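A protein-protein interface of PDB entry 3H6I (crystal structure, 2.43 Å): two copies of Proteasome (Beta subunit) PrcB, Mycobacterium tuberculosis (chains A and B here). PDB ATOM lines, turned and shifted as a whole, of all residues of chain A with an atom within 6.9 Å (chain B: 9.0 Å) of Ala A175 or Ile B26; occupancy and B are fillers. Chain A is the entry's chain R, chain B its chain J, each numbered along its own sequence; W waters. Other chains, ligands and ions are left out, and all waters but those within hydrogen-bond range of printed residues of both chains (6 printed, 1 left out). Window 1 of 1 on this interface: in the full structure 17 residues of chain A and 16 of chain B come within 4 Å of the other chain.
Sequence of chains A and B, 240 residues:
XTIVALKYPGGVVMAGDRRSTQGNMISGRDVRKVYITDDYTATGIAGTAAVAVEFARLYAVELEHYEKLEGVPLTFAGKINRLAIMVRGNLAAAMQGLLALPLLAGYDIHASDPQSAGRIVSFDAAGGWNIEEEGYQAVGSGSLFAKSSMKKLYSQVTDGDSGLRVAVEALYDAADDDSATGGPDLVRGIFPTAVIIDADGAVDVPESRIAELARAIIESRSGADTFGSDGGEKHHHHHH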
ATOM      1  N   THR A   2      18.525 -20.838 -20.123  1.00  0.00           N
ATOM      2  CA  THR A   2      18.793 -22.226 -20.535  1.00  0.00           C
ATOM      3  C   THR A   2      17.923 -23.258 -19.847  1.00  0.00           C
ATOM      4  O   THR A   2      17.641 -23.164 -18.658  1.00  0.00           O
ATOM      5  CB  THR A   2      20.272 -22.592 -20.332  1.00  0.00           C
ATOM      6  OG1 THR A   2      21.094 -21.586 -20.927  1.00  0.00           O
ATOM      7  CG2 THR A   2      20.632 -23.959 -20.973  1.00  0.00           C
ATOM      8  N   ASP A  17      17.206 -22.522 -15.530  1.00  0.00           N
ATOM      9  CA  ASP A  17      17.771 -21.405 -14.759  1.00  0.00           C
ATOM     10  C   ASP A  17      16.622 -20.436 -14.322  1.00  0.00           C
ATOM     11  O   ASP A  17      15.439 -20.587 -14.720  1.00  0.00           O
ATOM     12  CB  ASP A  17      18.862 -20.671 -15.575  1.00  0.00           C
ATOM     13  CG  ASP A  17      18.280 -19.596 -16.550  1.00  0.00           C
ATOM     14  OD1 ASP A  17      17.456 -19.933 -17.442  1.00  0.00           O
ATOM     15  OD2 ASP A  17      18.600 -18.404 -16.351  1.00  0.00           O
ATOM     16  N   ARG A  19      16.940 -16.702 -14.531  1.00  0.00           N
ATOM     17  CA  ARG A  19      17.109 -15.334 -14.966  1.00  0.00           C
ATOM     18  C   ARG A  19      16.182 -14.932 -16.104  1.00  0.00           C
ATOM     19  O   ARG A  19      15.616 -15.768 -16.762  1.00  0.00           O
ATOM     20  CB  ARG A  19      18.562 -15.168 -15.426  1.00  0.00           C
ATOM     21  CG  ARG A  19      18.997 -13.827 -15.993  1.00  0.00           C
ATOM     22  CD  ARG A  19      20.524 -13.688 -16.073  1.00  0.00           C
ATOM     23  NE  ARG A  19      21.081 -13.558 -14.734  1.00  0.00           N
ATOM     24  CZ  ARG A  19      22.355 -13.292 -14.467  1.00  0.00           C
ATOM     25  NH1 ARG A  19      23.247 -13.134 -15.436  1.00  0.00           N
ATOM     26  NH2 ARG A  19      22.744 -13.154 -13.213  1.00  0.00           N
ATOM     27  N   GLY A 142      22.085 -20.431 -23.642  1.00  0.00           N
ATOM     28  CA  GLY A 142      23.250 -21.110 -23.098  1.00  0.00           C
ATOM     29  C   GLY A 142      23.265 -22.565 -23.482  1.00  0.00           C
ATOM     30  O   GLY A 142      24.153 -23.344 -23.058  1.00  0.00           O
ATOM     31  N   PHE A 145      26.569 -24.319 -24.640  1.00  0.00           N
ATOM     32  CA  PHE A 145      27.505 -24.520 -23.538  1.00  0.00           C
ATOM     33  C   PHE A 145      27.047 -25.670 -22.626  1.00  0.00           C
ATOM     34  O   PHE A 145      27.872 -26.524 -22.284  1.00  0.00           O
ATOM     35  CB  PHE A 145      27.650 -23.265 -22.773  1.00  0.00           C
ATOM     36  CG  PHE A 145      28.151 -22.129 -23.596  1.00  0.00           C
ATOM     37  CD1 PHE A 145      29.440 -22.156 -24.152  1.00  0.00           C
ATOM     38  CD2 PHE A 145      27.379 -20.965 -23.714  1.00  0.00           C
ATOM     39  CE1 PHE A 145      29.964 -21.009 -24.817  1.00  0.00           C
ATOM     40  CE2 PHE A 145      27.884 -19.808 -24.374  1.00  0.00           C
ATOM     41  CZ  PHE A 145      29.178 -19.834 -24.923  1.00  0.00           C
ATOM     42  N   GLU A 169      24.944 -29.115 -13.244  1.00  0.00           N
ATOM     43  CA  GLU A 169      26.284 -28.704 -13.670  1.00  0.00           C
ATOM     44  C   GLU A 169      26.217 -28.116 -15.087  1.00  0.00           C
ATOM     45  O   GLU A 169      26.892 -27.148 -15.352  1.00  0.00           O
ATOM     46  CB  GLU A 169      27.285 -29.887 -13.601  1.00  0.00           C
ATOM     47  CG  GLU A 169      28.745 -29.482 -13.764  1.00  0.00           C
ATOM     48  CD  GLU A 169      29.742 -30.562 -13.298  1.00  0.00           C
ATOM     49  OE1 GLU A 169      29.306 -31.558 -12.644  1.00  0.00           O
ATOM     50  OE2 GLU A 169      30.960 -30.419 -13.597  1.00  0.00           O
ATOM     51  N   ALA A 170      25.407 -28.704 -15.982  1.00  0.00           N
ATOM     52  CA  ALA A 170      25.228 -28.194 -17.341  1.00  0.00           C
ATOM     53  C   ALA A 170      24.676 -26.736 -17.300  1.00  0.00           C
ATOM     54  O   ALA A 170      25.181 -25.884 -18.015  1.00  0.00           O
ATOM     55  CB  ALA A 170      24.273 -29.117 -18.167  1.00  0.00           C
ATOM     56  N   LEU A 171      23.718 -26.461 -16.397  1.00  0.00           N
ATOM     57  CA  LEU A 171      23.150 -25.100 -16.220  1.00  0.00           C
ATOM     58  C   LEU A 171      24.208 -24.149 -15.684  1.00  0.00           C
ATOM     59  O   LEU A 171      24.281 -22.978 -16.095  1.00  0.00           O
ATOM     60  CB  LEU A 171      21.934 -25.091 -15.273  1.00  0.00           C
ATOM     61  CG  LEU A 171      20.693 -25.662 -15.931  1.00  0.00           C
ATOM     62  CD1 LEU A 171      19.614 -25.613 -14.937  1.00  0.00           C
ATOM     63  CD2 LEU A 171      20.272 -24.808 -17.115  1.00  0.00           C
ATOM     64  N   TYR A 172      25.074 -24.687 -14.816  1.00  0.00           N
ATOM     65  CA  TYR A 172      26.150 -23.919 -14.229  1.00  0.00           C
ATOM     66  C   TYR A 172      27.122 -23.540 -15.327  1.00  0.00           C
ATOM     67  O   TYR A 172      27.646 -22.419 -15.354  1.00  0.00           O
ATOM     68  CB  TYR A 172      26.873 -24.742 -13.152  1.00  0.00           C
ATOM     69  CG  TYR A 172      27.962 -23.997 -12.434  1.00  0.00           C
ATOM     70  CD1 TYR A 172      27.643 -23.197 -11.318  1.00  0.00           C
ATOM     71  CD2 TYR A 172      29.270 -24.019 -12.882  1.00  0.00           C
ATOM     72  CE1 TYR A 172      28.591 -22.436 -10.674  1.00  0.00           C
ATOM     73  CE2 TYR A 172      30.268 -23.245 -12.224  1.00  0.00           C
ATOM     74  CZ  TYR A 172      29.911 -22.470 -11.126  1.00  0.00           C
ATOM     75  OH  TYR A 172      30.863 -21.740 -10.473  1.00  0.00           O
ATOM     76  N   ASP A 173      27.413 -24.493 -16.205  1.00  0.00           N
ATOM     77  CA  ASP A 173      28.333 -24.225 -17.299  1.00  0.00           C
ATOM     78  C   ASP A 173      27.739 -23.244 -18.314  1.00  0.00           C
ATOM     79  O   ASP A 173      28.466 -22.428 -18.870  1.00  0.00           O
ATOM     80  CB  ASP A 173      28.792 -25.506 -17.970  1.00  0.00           C
ATOM     81  CG  ASP A 173      29.969 -26.149 -17.230  1.00  0.00           C
ATOM     82  OD1 ASP A 173      30.909 -25.424 -16.826  1.00  0.00           O
ATOM     83  OD2 ASP A 173      29.954 -27.382 -17.047  1.00  0.00           O
ATOM     84  N   ALA A 174      26.416 -23.299 -18.510  1.00  0.00           N
ATOM     85  CA  ALA A 174      25.711 -22.382 -19.407  1.00  0.00           C
ATOM     86  C   ALA A 174      25.842 -20.987 -18.805  1.00  0.00           C
ATOM     87  O   ALA A 174      26.246 -20.090 -19.510  1.00  0.00           O
ATOM     88  CB  ALA A 174      24.217 -22.749 -19.555  1.00  0.00           C
ATOM     89  N   ALA A 175      25.638 -20.844 -17.484  1.00  0.00           N
ATOM     90  CA  ALA A 175      25.770 -19.512 -16.839  1.00  0.00           C
ATOM     91  C   ALA A 175      27.165 -18.968 -16.834  1.00  0.00           C
ATOM     92  O   ALA A 175      27.353 -17.764 -16.928  1.00  0.00           O
ATOM     93  CB  ALA A 175      25.258 -19.509 -15.447  1.00  0.00           C
ATOM     94  N   ASP A 176      28.133 -19.865 -16.749  1.00  0.00           N
ATOM     95  CA  ASP A 176      29.525 -19.521 -16.718  1.00  0.00           C
ATOM     96  C   ASP A 176      29.981 -18.892 -18.000  1.00  0.00           C
ATOM     97  O   ASP A 176      30.834 -18.059 -18.016  1.00  0.00           O
ATOM     98  CB  ASP A 176      30.359 -20.751 -16.438  1.00  0.00           C
ATOM     99  CG  ASP A 176      31.617 -20.442 -15.694  1.00  0.00           C
ATOM    100  OD1 ASP A 176      31.703 -19.400 -15.083  1.00  0.00           O
ATOM    101  OD2 ASP A 176      32.516 -21.262 -15.695  1.00  0.00           O
ATOM    102  N   ASP A 177      29.369 -19.288 -19.079  1.00  0.00           N
ATOM    103  CA  ASP A 177      29.739 -18.737 -20.377  1.00  0.00           C
ATOM    104  C   ASP A 177      28.699 -17.834 -21.072  1.00  0.00           C
ATOM    105  O   ASP A 177      28.979 -17.171 -22.064  1.00  0.00           O
ATOM    106  CB  ASP A 177      30.198 -19.882 -21.292  1.00  0.00           C
ATOM    107  CG  ASP A 177      31.546 -20.523 -20.840  1.00  0.00           C
ATOM    108  OD1 ASP A 177      32.470 -19.797 -20.425  1.00  0.00           O
ATOM    109  OD2 ASP A 177      31.690 -21.758 -20.898  1.00  0.00           O
ATOM    110  N   ASP A 178      27.479 -17.856 -20.572  1.00  0.00           N
ATOM    111  CA  ASP A 178      26.409 -17.061 -21.115  1.00  0.00           C
ATOM    112  C   ASP A 178      25.803 -16.115 -20.030  1.00  0.00           C
ATOM    113  O   ASP A 178      25.016 -16.534 -19.186  1.00  0.00           O
ATOM    114  CB  ASP A 178      25.355 -18.001 -21.727  1.00  0.00           C
ATOM    115  CG  ASP A 178      24.063 -17.275 -22.129  1.00  0.00           C
ATOM    116  OD1 ASP A 178      24.130 -16.122 -22.597  1.00  0.00           O
ATOM    117  OD2 ASP A 178      22.986 -17.852 -21.933  1.00  0.00           O
ATOM    118  N   SER A 179      25.997 -14.814 -20.233  1.00  0.00           N
ATOM    119  CA  SER A 179      25.497 -13.791 -19.312  1.00  0.00           C
ATOM    120  C   SER A 179      23.975 -13.708 -19.250  1.00  0.00           C
ATOM    121  O   SER A 179      23.414 -13.208 -18.280  1.00  0.00           O
ATOM    122  CB  SER A 179      26.127 -12.438 -19.646  1.00  0.00           C
ATOM    123  OG  SER A 179      25.631 -11.933 -20.852  1.00  0.00           O
ATOM    124  N   ALA A 180      23.302 -14.337 -20.211  1.00  0.00           N
ATOM    125  CA  ALA A 180      21.836 -14.331 -20.217  1.00  0.00           C
ATOM    126  C   ALA A 180      21.279 -15.515 -19.403  1.00  0.00           C
ATOM    127  O   ALA A 180      20.073 -15.621 -19.207  1.00  0.00           O
ATOM    128  CB  ALA A 180      21.306 -14.366 -21.667  1.00  0.00           C
ATOM    129  N   THR A 181      22.148 -16.420 -18.966  1.00  0.00           N
ATOM    130  CA  THR A 181      21.695 -17.570 -18.131  1.00  0.00           C
ATOM    131  C   THR A 181      22.147 -17.348 -16.709  1.00  0.00           C
ATOM    132  O   THR A 181      23.316 -17.006 -16.495  1.00  0.00           O
ATOM    133  CB  THR A 181      22.245 -18.896 -18.681  1.00  0.00           C
ATOM    134  OG1 THR A 181      21.705 -19.065 -19.997  1.00  0.00           O
ATOM    135  CG2 THR A 181      21.845 -20.109 -17.814  1.00  0.00           C
ATOM    136  N   GLY A 182      21.213 -17.466 -15.752  1.00  0.00           N
ATOM    137  CA  GLY A 182      21.565 -17.240 -14.351  1.00  0.00           C
ATOM    138  C   GLY A 182      22.207 -18.385 -13.562  1.00  0.00           C
ATOM    139  O   GLY A 182      21.694 -19.478 -13.569  1.00  0.00           O
ATOM    140  N   GLY A 183      23.363 -18.139 -12.938  1.00  0.00           N
ATOM    141  CA  GLY A 183      23.980 -19.157 -12.106  1.00  0.00           C
ATOM    142  C   GLY A 183      23.336 -19.229 -10.731  1.00  0.00           C
ATOM    143  O   GLY A 183      22.440 -18.418 -10.419  1.00  0.00           O
ATOM    144  N   PRO A 184      23.713 -20.210  -9.887  1.00  0.00           N
ATOM    145  CA  PRO A 184      23.163 -20.356  -8.521  1.00  0.00           C
ATOM    146  C   PRO A 184      23.480 -19.061  -7.775  1.00  0.00           C
ATOM    147  O   PRO A 184      24.543 -18.490  -7.988  1.00  0.00           O
ATOM    148  CB  PRO A 184      23.986 -21.493  -7.967  1.00  0.00           C
ATOM    149  CG  PRO A 184      24.236 -22.351  -9.185  1.00  0.00           C
ATOM    150  CD  PRO A 184      24.649 -21.301 -10.182  1.00  0.00           C
ATOM    151  N   ARG B  18      35.816  -6.803 -14.610  1.00  0.00           N
ATOM    152  CA  ARG B  18      36.720  -7.632 -15.410  1.00  0.00           C
ATOM    153  C   ARG B  18      36.110  -8.375 -16.564  1.00  0.00           C
ATOM    154  O   ARG B  18      36.802  -9.165 -17.213  1.00  0.00           O
ATOM    155  CB  ARG B  18      37.345  -8.687 -14.469  1.00  0.00           C
ATOM    156  CG  ARG B  18      37.998  -8.179 -13.158  1.00  0.00           C
ATOM    157  CD  ARG B  18      39.101  -7.101 -13.378  1.00  0.00           C
ATOM    158  NE  ARG B  18      40.248  -7.680 -14.043  1.00  0.00           N
ATOM    159  CZ  ARG B  18      41.231  -8.337 -13.431  1.00  0.00           C
ATOM    160  NH1 ARG B  18      41.206  -8.501 -12.101  1.00  0.00           N
ATOM    161  NH2 ARG B  18      42.275  -8.766 -14.139  1.00  0.00           N
ATOM    162  N   ARG B  19      34.831  -8.153 -16.809  1.00  0.00           N
ATOM    163  CA  ARG B  19      34.097  -8.816 -17.874  1.00  0.00           C
ATOM    164  C   ARG B  19      34.273  -8.207 -19.259  1.00  0.00           C
ATOM    165  O   ARG B  19      34.630  -7.057 -19.388  1.00  0.00           O
ATOM    166  CB  ARG B  19      32.621  -8.861 -17.512  1.00  0.00           C
ATOM    167  CG  ARG B  19      31.776  -9.667 -18.443  1.00  0.00           C
ATOM    168  CD  ARG B  19      30.471 -10.043 -17.810  1.00  0.00           C
ATOM    169  NE  ARG B  19      30.639 -11.123 -16.863  1.00  0.00           N
ATOM    170  CZ  ARG B  19      29.647 -11.742 -16.251  1.00  0.00           C
ATOM    171  NH1 ARG B  19      28.399 -11.394 -16.477  1.00  0.00           N
ATOM    172  NH2 ARG B  19      29.909 -12.711 -15.408  1.00  0.00           N
ATOM    173  N   SER B  20      34.013  -9.014 -20.281  1.00  0.00           N
ATOM    174  CA  SER B  20      33.911  -8.572 -21.688  1.00  0.00           C
ATOM    175  C   SER B  20      32.947  -9.599 -22.272  1.00  0.00           C
ATOM    176  O   SER B  20      32.915 -10.791 -21.872  1.00  0.00           O
ATOM    177  CB  SER B  20      35.258  -8.471 -22.447  1.00  0.00           C
ATOM    178  OG  SER B  20      35.755  -9.737 -22.832  1.00  0.00           O
ATOM    179  N   THR B  21      32.038  -9.090 -23.077  1.00  0.00           N
ATOM    180  CA  THR B  21      31.025  -9.899 -23.716  1.00  0.00           C
ATOM    181  C   THR B  21      30.967  -9.708 -25.231  1.00  0.00           C
ATOM    182  O   THR B  21      31.400  -8.696 -25.754  1.00  0.00           O
ATOM    183  CB  THR B  21      29.600  -9.597 -23.139  1.00  0.00           C
ATOM    184  OG1 THR B  21      29.314  -8.184 -23.191  1.00  0.00           O
ATOM    185  CG2 THR B  21      29.426 -10.139 -21.725  1.00  0.00           C
ATOM    186  N   GLN B  22      30.450 -10.707 -25.928  1.00  0.00           N
ATOM    187  CA  GLN B  22      30.249 -10.648 -27.372  1.00  0.00           C
ATOM    188  C   GLN B  22      28.784 -11.095 -27.447  1.00  0.00           C
ATOM    189  O   GLN B  22      28.479 -12.299 -27.367  1.00  0.00           O
ATOM    190  CB  GLN B  22      31.182 -11.603 -28.081  1.00  0.00           C
ATOM    191  CG  GLN B  22      31.388 -11.257 -29.519  1.00  0.00           C
ATOM    192  CD  GLN B  22      32.607 -11.954 -30.053  1.00  0.00           C
ATOM    193  OE1 GLN B  22      33.751 -11.606 -29.700  1.00  0.00           O
ATOM    194  NE2 GLN B  22      32.381 -12.978 -30.875  1.00  0.00           N
ATOM    195  N   GLY B  23      27.889 -10.098 -27.439  1.00  0.00           N
ATOM    196  CA  GLY B  23      26.456 -10.349 -27.408  1.00  0.00           C
ATOM    197  C   GLY B  23      26.157 -10.886 -26.003  1.00  0.00           C
ATOM    198  O   GLY B  23      26.605 -10.296 -25.015  1.00  0.00           O
ATOM    199  N   ASN B  24      25.554 -12.075 -25.926  1.00  0.00           N
ATOM    200  CA  ASN B  24      25.263 -12.702 -24.622  1.00  0.00           C
ATOM    201  C   ASN B  24      26.456 -13.503 -24.038  1.00  0.00           C
ATOM    202  O   ASN B  24      26.487 -13.785 -22.845  1.00  0.00           O
ATOM    203  CB  ASN B  24      24.051 -13.640 -24.738  1.00  0.00           C
ATOM    204  CG  ASN B  24      22.725 -12.893 -24.825  1.00  0.00           C
ATOM    205  OD1 ASN B  24      22.509 -11.849 -24.161  1.00  0.00           O
ATOM    206  ND2 ASN B  24      21.809 -13.450 -25.624  1.00  0.00           N
ATOM    207  N   MET B  25      27.456 -13.788 -24.873  1.00  0.00           N
ATOM    208  CA  MET B  25      28.618 -14.585 -24.483  1.00  0.00           C
ATOM    209  C   MET B  25      29.722 -13.907 -23.698  1.00  0.00           C
ATOM    210  O   MET B  25      30.181 -12.841 -24.044  1.00  0.00           O
ATOM    211  CB  MET B  25      29.239 -15.299 -25.698  1.00  0.00           C
ATOM    212  CG  MET B  25      28.255 -16.235 -26.421  1.00  0.00           C
ATOM    213  SD  MET B  25      29.004 -16.925 -27.891  1.00  0.00           S
ATOM    214  CE  MET B  25      28.726 -15.501 -29.123  1.00  0.00           C
ATOM    215  N   ILE B  26      30.159 -14.563 -22.655  1.00  0.00           N
ATOM    216  CA  ILE B  26      31.252 -14.063 -21.904  1.00  0.00           C
ATOM    217  C   ILE B  26      32.524 -14.352 -22.661  1.00  0.00           C
ATOM    218  O   ILE B  26      32.901 -15.453 -22.800  1.00  0.00           O
ATOM    219  CB  ILE B  26      31.241 -14.633 -20.489  1.00  0.00           C
ATOM    220  CG1 ILE B  26      30.055 -14.052 -19.739  1.00  0.00           C
ATOM    221  CG2 ILE B  26      32.493 -14.300 -19.783  1.00  0.00           C
ATOM    222  CD1 ILE B  26      29.394 -14.958 -18.810  1.00  0.00           C
ATOM    223  N   SER B  27      33.165 -13.339 -23.186  1.00  0.00           N
ATOM    224  CA  SER B  27      34.419 -13.509 -23.921  1.00  0.00           C
ATOM    225  C   SER B  27      35.686 -13.258 -23.065  1.00  0.00           C
ATOM    226  O   SER B  27      36.794 -13.574 -23.498  1.00  0.00           O
ATOM    227  CB  SER B  27      34.444 -12.597 -25.146  1.00  0.00           C
ATOM    228  OG  SER B  27      34.214 -11.252 -24.775  1.00  0.00           O
ATOM    229  N   GLY B  28      35.522 -12.711 -21.858  1.00  0.00           N
ATOM    230  CA  GLY B  28      36.679 -12.402 -21.017  1.00  0.00           C
ATOM    231  C   GLY B  28      36.283 -12.302 -19.571  1.00  0.00           C
ATOM    232  O   GLY B  28      35.149 -11.914 -19.231  1.00  0.00           O
ATOM    233  N   ARG B  29      37.207 -12.681 -18.702  1.00  0.00           N
ATOM    234  CA  ARG B  29      36.992 -12.679 -17.268  1.00  0.00           C
ATOM    235  C   ARG B  29      38.057 -11.930 -16.496  1.00  0.00           C
ATOM    236  O   ARG B  29      37.911 -11.732 -15.335  1.00  0.00           O
ATOM    237  CB  ARG B  29      36.939 -14.094 -16.727  1.00  0.00           C
ATOM    238  CG  ARG B  29      35.916 -14.964 -17.311  1.00  0.00           C
ATOM    239  CD  ARG B  29      35.894 -16.318 -16.703  1.00  0.00           C
ATOM    240  NE  ARG B  29      34.690 -16.988 -17.099  1.00  0.00           N
ATOM    241  CZ  ARG B  29      34.597 -17.765 -18.148  1.00  0.00           C
ATOM    242  NH1 ARG B  29      35.646 -17.995 -18.873  1.00  0.00           N
ATOM    243  NH2 ARG B  29      33.461 -18.309 -18.465  1.00  0.00           N
ATOM    244  N   ASP B  30      39.135 -11.532 -17.130  1.00  0.00           N
ATOM    245  CA  ASP B  30      40.236 -10.856 -16.420  1.00  0.00           C
ATOM    246  C   ASP B  30      40.653  -9.577 -17.113  1.00  0.00           C
ATOM    247  O   ASP B  30      41.796  -9.178 -17.028  1.00  0.00           O
ATOM    248  CB  ASP B  30      41.455 -11.797 -16.251  1.00  0.00           C
ATOM    249  CG  ASP B  30      41.835 -12.533 -17.555  1.00  0.00           C
ATOM    250  OD1 ASP B  30      41.876 -13.792 -17.549  1.00  0.00           O
ATOM    251  OD2 ASP B  30      42.080 -11.857 -18.582  1.00  0.00           O
ATOM    252  N   VAL B  31      39.707  -8.949 -17.795  1.00  0.00           N
ATOM    253  CA  VAL B  31      39.961  -7.725 -18.517  1.00  0.00           C
ATOM    254  C   VAL B  31      40.347  -6.580 -17.551  1.00  0.00           C
ATOM    255  O   VAL B  31      39.710  -6.338 -16.530  1.00  0.00           O
ATOM    256  CB  VAL B  31      38.713  -7.371 -19.412  1.00  0.00           C
ATOM    257  CG1 VAL B  31      38.953  -6.146 -20.244  1.00  0.00           C
ATOM    258  CG2 VAL B  31      38.375  -8.526 -20.324  1.00  0.00           C
ATOM    259  N   SER B 179      24.030  -7.680 -16.529  1.00  0.00           N
ATOM    260  CA  SER B 179      24.687  -8.904 -16.956  1.00  0.00           C
ATOM    261  C   SER B 179      25.937  -8.671 -17.733  1.00  0.00           C
ATOM    262  O   SER B 179      26.745  -9.585 -17.850  1.00  0.00           O
ATOM    263  CB  SER B 179      23.717  -9.810 -17.732  1.00  0.00           C
ATOM    264  OG  SER B 179      23.464  -9.290 -19.013  1.00  0.00           O
ATOM    265  N   ALA B 180      26.154  -7.430 -18.175  1.00  0.00           N
ATOM    266  CA  ALA B 180      27.355  -7.137 -18.958  1.00  0.00           C
ATOM    267  C   ALA B 180      28.497  -6.723 -18.045  1.00  0.00           C
ATOM    268  O   ALA B 180      29.634  -6.592 -18.481  1.00  0.00           O
ATOM    269  CB  ALA B 180      27.100  -6.081 -20.057  1.00  0.00           C
ATOM    270  N   THR B 181      28.197  -6.530 -16.774  1.00  0.00           N
ATOM    271  CA  THR B 181      29.254  -6.185 -15.807  1.00  0.00           C
ATOM    272  C   THR B 181      29.596  -7.426 -14.934  1.00  0.00           C
ATOM    273  O   THR B 181      28.707  -8.129 -14.419  1.00  0.00           O
ATOM    274  CB  THR B 181      28.804  -4.987 -14.972  1.00  0.00           C
ATOM    275  OG1 THR B 181      28.598  -3.891 -15.860  1.00  0.00           O
ATOM    276  CG2 THR B 181      29.858  -4.595 -13.875  1.00  0.00           C
ATOM    277  N   GLY B 182      30.873  -7.754 -14.824  1.00  0.00           N
ATOM    278  CA  GLY B 182      31.218  -8.932 -14.015  1.00  0.00           C
ATOM    279  C   GLY B 182      31.348  -8.701 -12.503  1.00  0.00           C
ATOM    280  O   GLY B 182      31.861  -7.683 -12.084  1.00  0.00           O
ATOM    281  N   ASP B 185      34.495 -12.945  -8.789  1.00  0.00           N
ATOM    282  CA  ASP B 185      34.437 -14.389  -9.072  1.00  0.00           C
ATOM    283  C   ASP B 185      35.267 -15.141  -7.978  1.00  0.00           C
ATOM    284  O   ASP B 185      36.497 -15.238  -8.046  1.00  0.00           O
ATOM    285  CB  ASP B 185      34.971 -14.653 -10.477  1.00  0.00           C
ATOM    286  CG  ASP B 185      34.853 -16.137 -10.914  1.00  0.00           C
ATOM    287  OD1 ASP B 185      34.603 -17.041 -10.067  1.00  0.00           O
ATOM    288  OD2 ASP B 185      34.992 -16.397 -12.140  1.00  0.00           O
ATOM    289  N   ARG B 188      37.249 -18.442  -9.263  1.00  0.00           N
ATOM    290  CA  ARG B 188      38.509 -18.181  -9.933  1.00  0.00           C
ATOM    291  C   ARG B 188      39.439 -17.194  -9.229  1.00  0.00           C
ATOM    292  O   ARG B 188      40.565 -17.029  -9.640  1.00  0.00           O
ATOM    293  CB  ARG B 188      38.245 -17.723 -11.366  1.00  0.00           C
ATOM    294  CG  ARG B 188      37.995 -18.859 -12.327  1.00  0.00           C
ATOM    295  CD  ARG B 188      37.565 -18.416 -13.714  1.00  0.00           C
ATOM    296  NE  ARG B 188      36.127 -18.358 -13.741  1.00  0.00           N
ATOM    297  CZ  ARG B 188      35.342 -19.121 -14.477  1.00  0.00           C
ATOM    298  NH1 ARG B 188      35.833 -19.989 -15.326  1.00  0.00           N
ATOM    299  NH2 ARG B 188      34.047 -18.972 -14.370  1.00  0.00           N
HETATM  300  O   HOH W   1      26.279 -12.758 -15.110  1.00  0.00           O
HETATM  301  O   HOH W   2      31.697 -17.707 -23.650  1.00  0.00           O
HETATM  302  O   HOH W   3      25.368  -9.089 -21.393  1.00  0.00           O
HETATM  303  O   HOH W   4      34.774 -21.020 -19.590  1.00  0.00           O
HETATM  304  O   HOH W   5      31.644 -17.170 -13.310  1.00  0.00           O
HETATM  305  O   HOH W   6      32.743 -21.117 -11.986  1.00  0.00           O
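N of Gly A142 lies within hydrogen-bond range of OD2 of Asp A178 (3.2 Å).
The backbone carbonyl oxygen of Ser B179 sits at hydrogen-bond distance from the guanidinium group of Arg B19.
NH1 of Arg A19 is in hydrogen-bond range of O of Ser A179 (2.8 Å).
The guanidinium group (NE) of Arg B188 lies within salt-bridge range of the side-chain carboxylate (OD2) of Asp B185.
Of the 21 printed residues of chain A, 6 touch a printed residue of chain B.
Along chain A the printed residues that touch a printed residue of chain B span positions 175 to 180.
Of the 20 printed residues of chain B, 6 touch a printed residue of chain A.
Hydrophobic or aromatic side chains of chain B that line the printed part of chain A: Ile B26.
Along chain B the printed residues that touch a printed residue of chain A span positions 24 to 188.
Among the printed residues, 13 pairs touch across the chains.
Among the printed residues, Asp or Glu carboxylates within 4 Å of a Lys or Arg side-chain nitrogen of the other chain: Asp A176 with Arg B29 (3.96 Å), Asp A176 with Arg B188 (2.5 Å) and Asp A177 with Arg B29 (2.7 Å).
Water W6 lies within hydrogen-bond range of the side-chain hydroxyl (OH) of Tyr A172 (2.5 Å) and the guanidinium group (NH2) of Arg B188 (3.5 Å).
Water W4 bridges the side-chain carboxylate of Asp A177 (2.7 Å) and the guanidinium group of Arg B29 (3.2 Å).
Among the printed residues, merely in contact across the chains: Ala A175 with Ile B26, Asp A176 with Ile B26, Asp A177 with Met B25, Asp A178 with Ile B26, Ser A179 with Ile B26, Ser A179 with Ser B179 and Ala A180 with Asn B24.
Ala A175 touches one residue of chain B.
Of chain A, only Ala A175, Asp A176, Asp A177, Asp A178 and Ser A179 come within 4 Å of Ile B26.
No residue of chain B comes within 4 Å of Gly A182.
Of the printed residues of chain B, Ala A180 touches Asn B24 (3.7 Å).
Of the printed residues of chain A, Met B25 touches Asp A177.
Phe A145 touches none of the printed residues of chain B.
Asp A173 touches none of the printed residues of chain B.
The nearest residue of chain A that does not touch Ile B26 is Phe A145 (5.8 Å).
The backbone NH of Ile B26 lies within hydrogen-bond range of the backbone carbonyl oxygen of Asp A177, 2.9 Å away.
The side-chain carboxylate (OD1) of Asp A176 is in salt-bridge range of the guanidinium group (NH2) of Arg B29, at 3.96 Å.
O of Asn B24 sits at hydrogen-bond distance from N of Ser A179, at 2.8 Å.
NH2 of Arg B29 lies within salt-bridge range of OD1 of Asp A177 (2.7 Å).
The side-chain carboxylate of Asp A176 lies within salt-bridge range of the guanidinium group of Arg B188 (2.5 Å).
The backbone carbonyl oxygen (O) of Asn B24 sits close to the side-chain carboxylate (OD1) of Asp A178, at 3.3 Å.
Ser B179 touches its own counterpart, Ser A179.
5 positions are printed for both chains.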
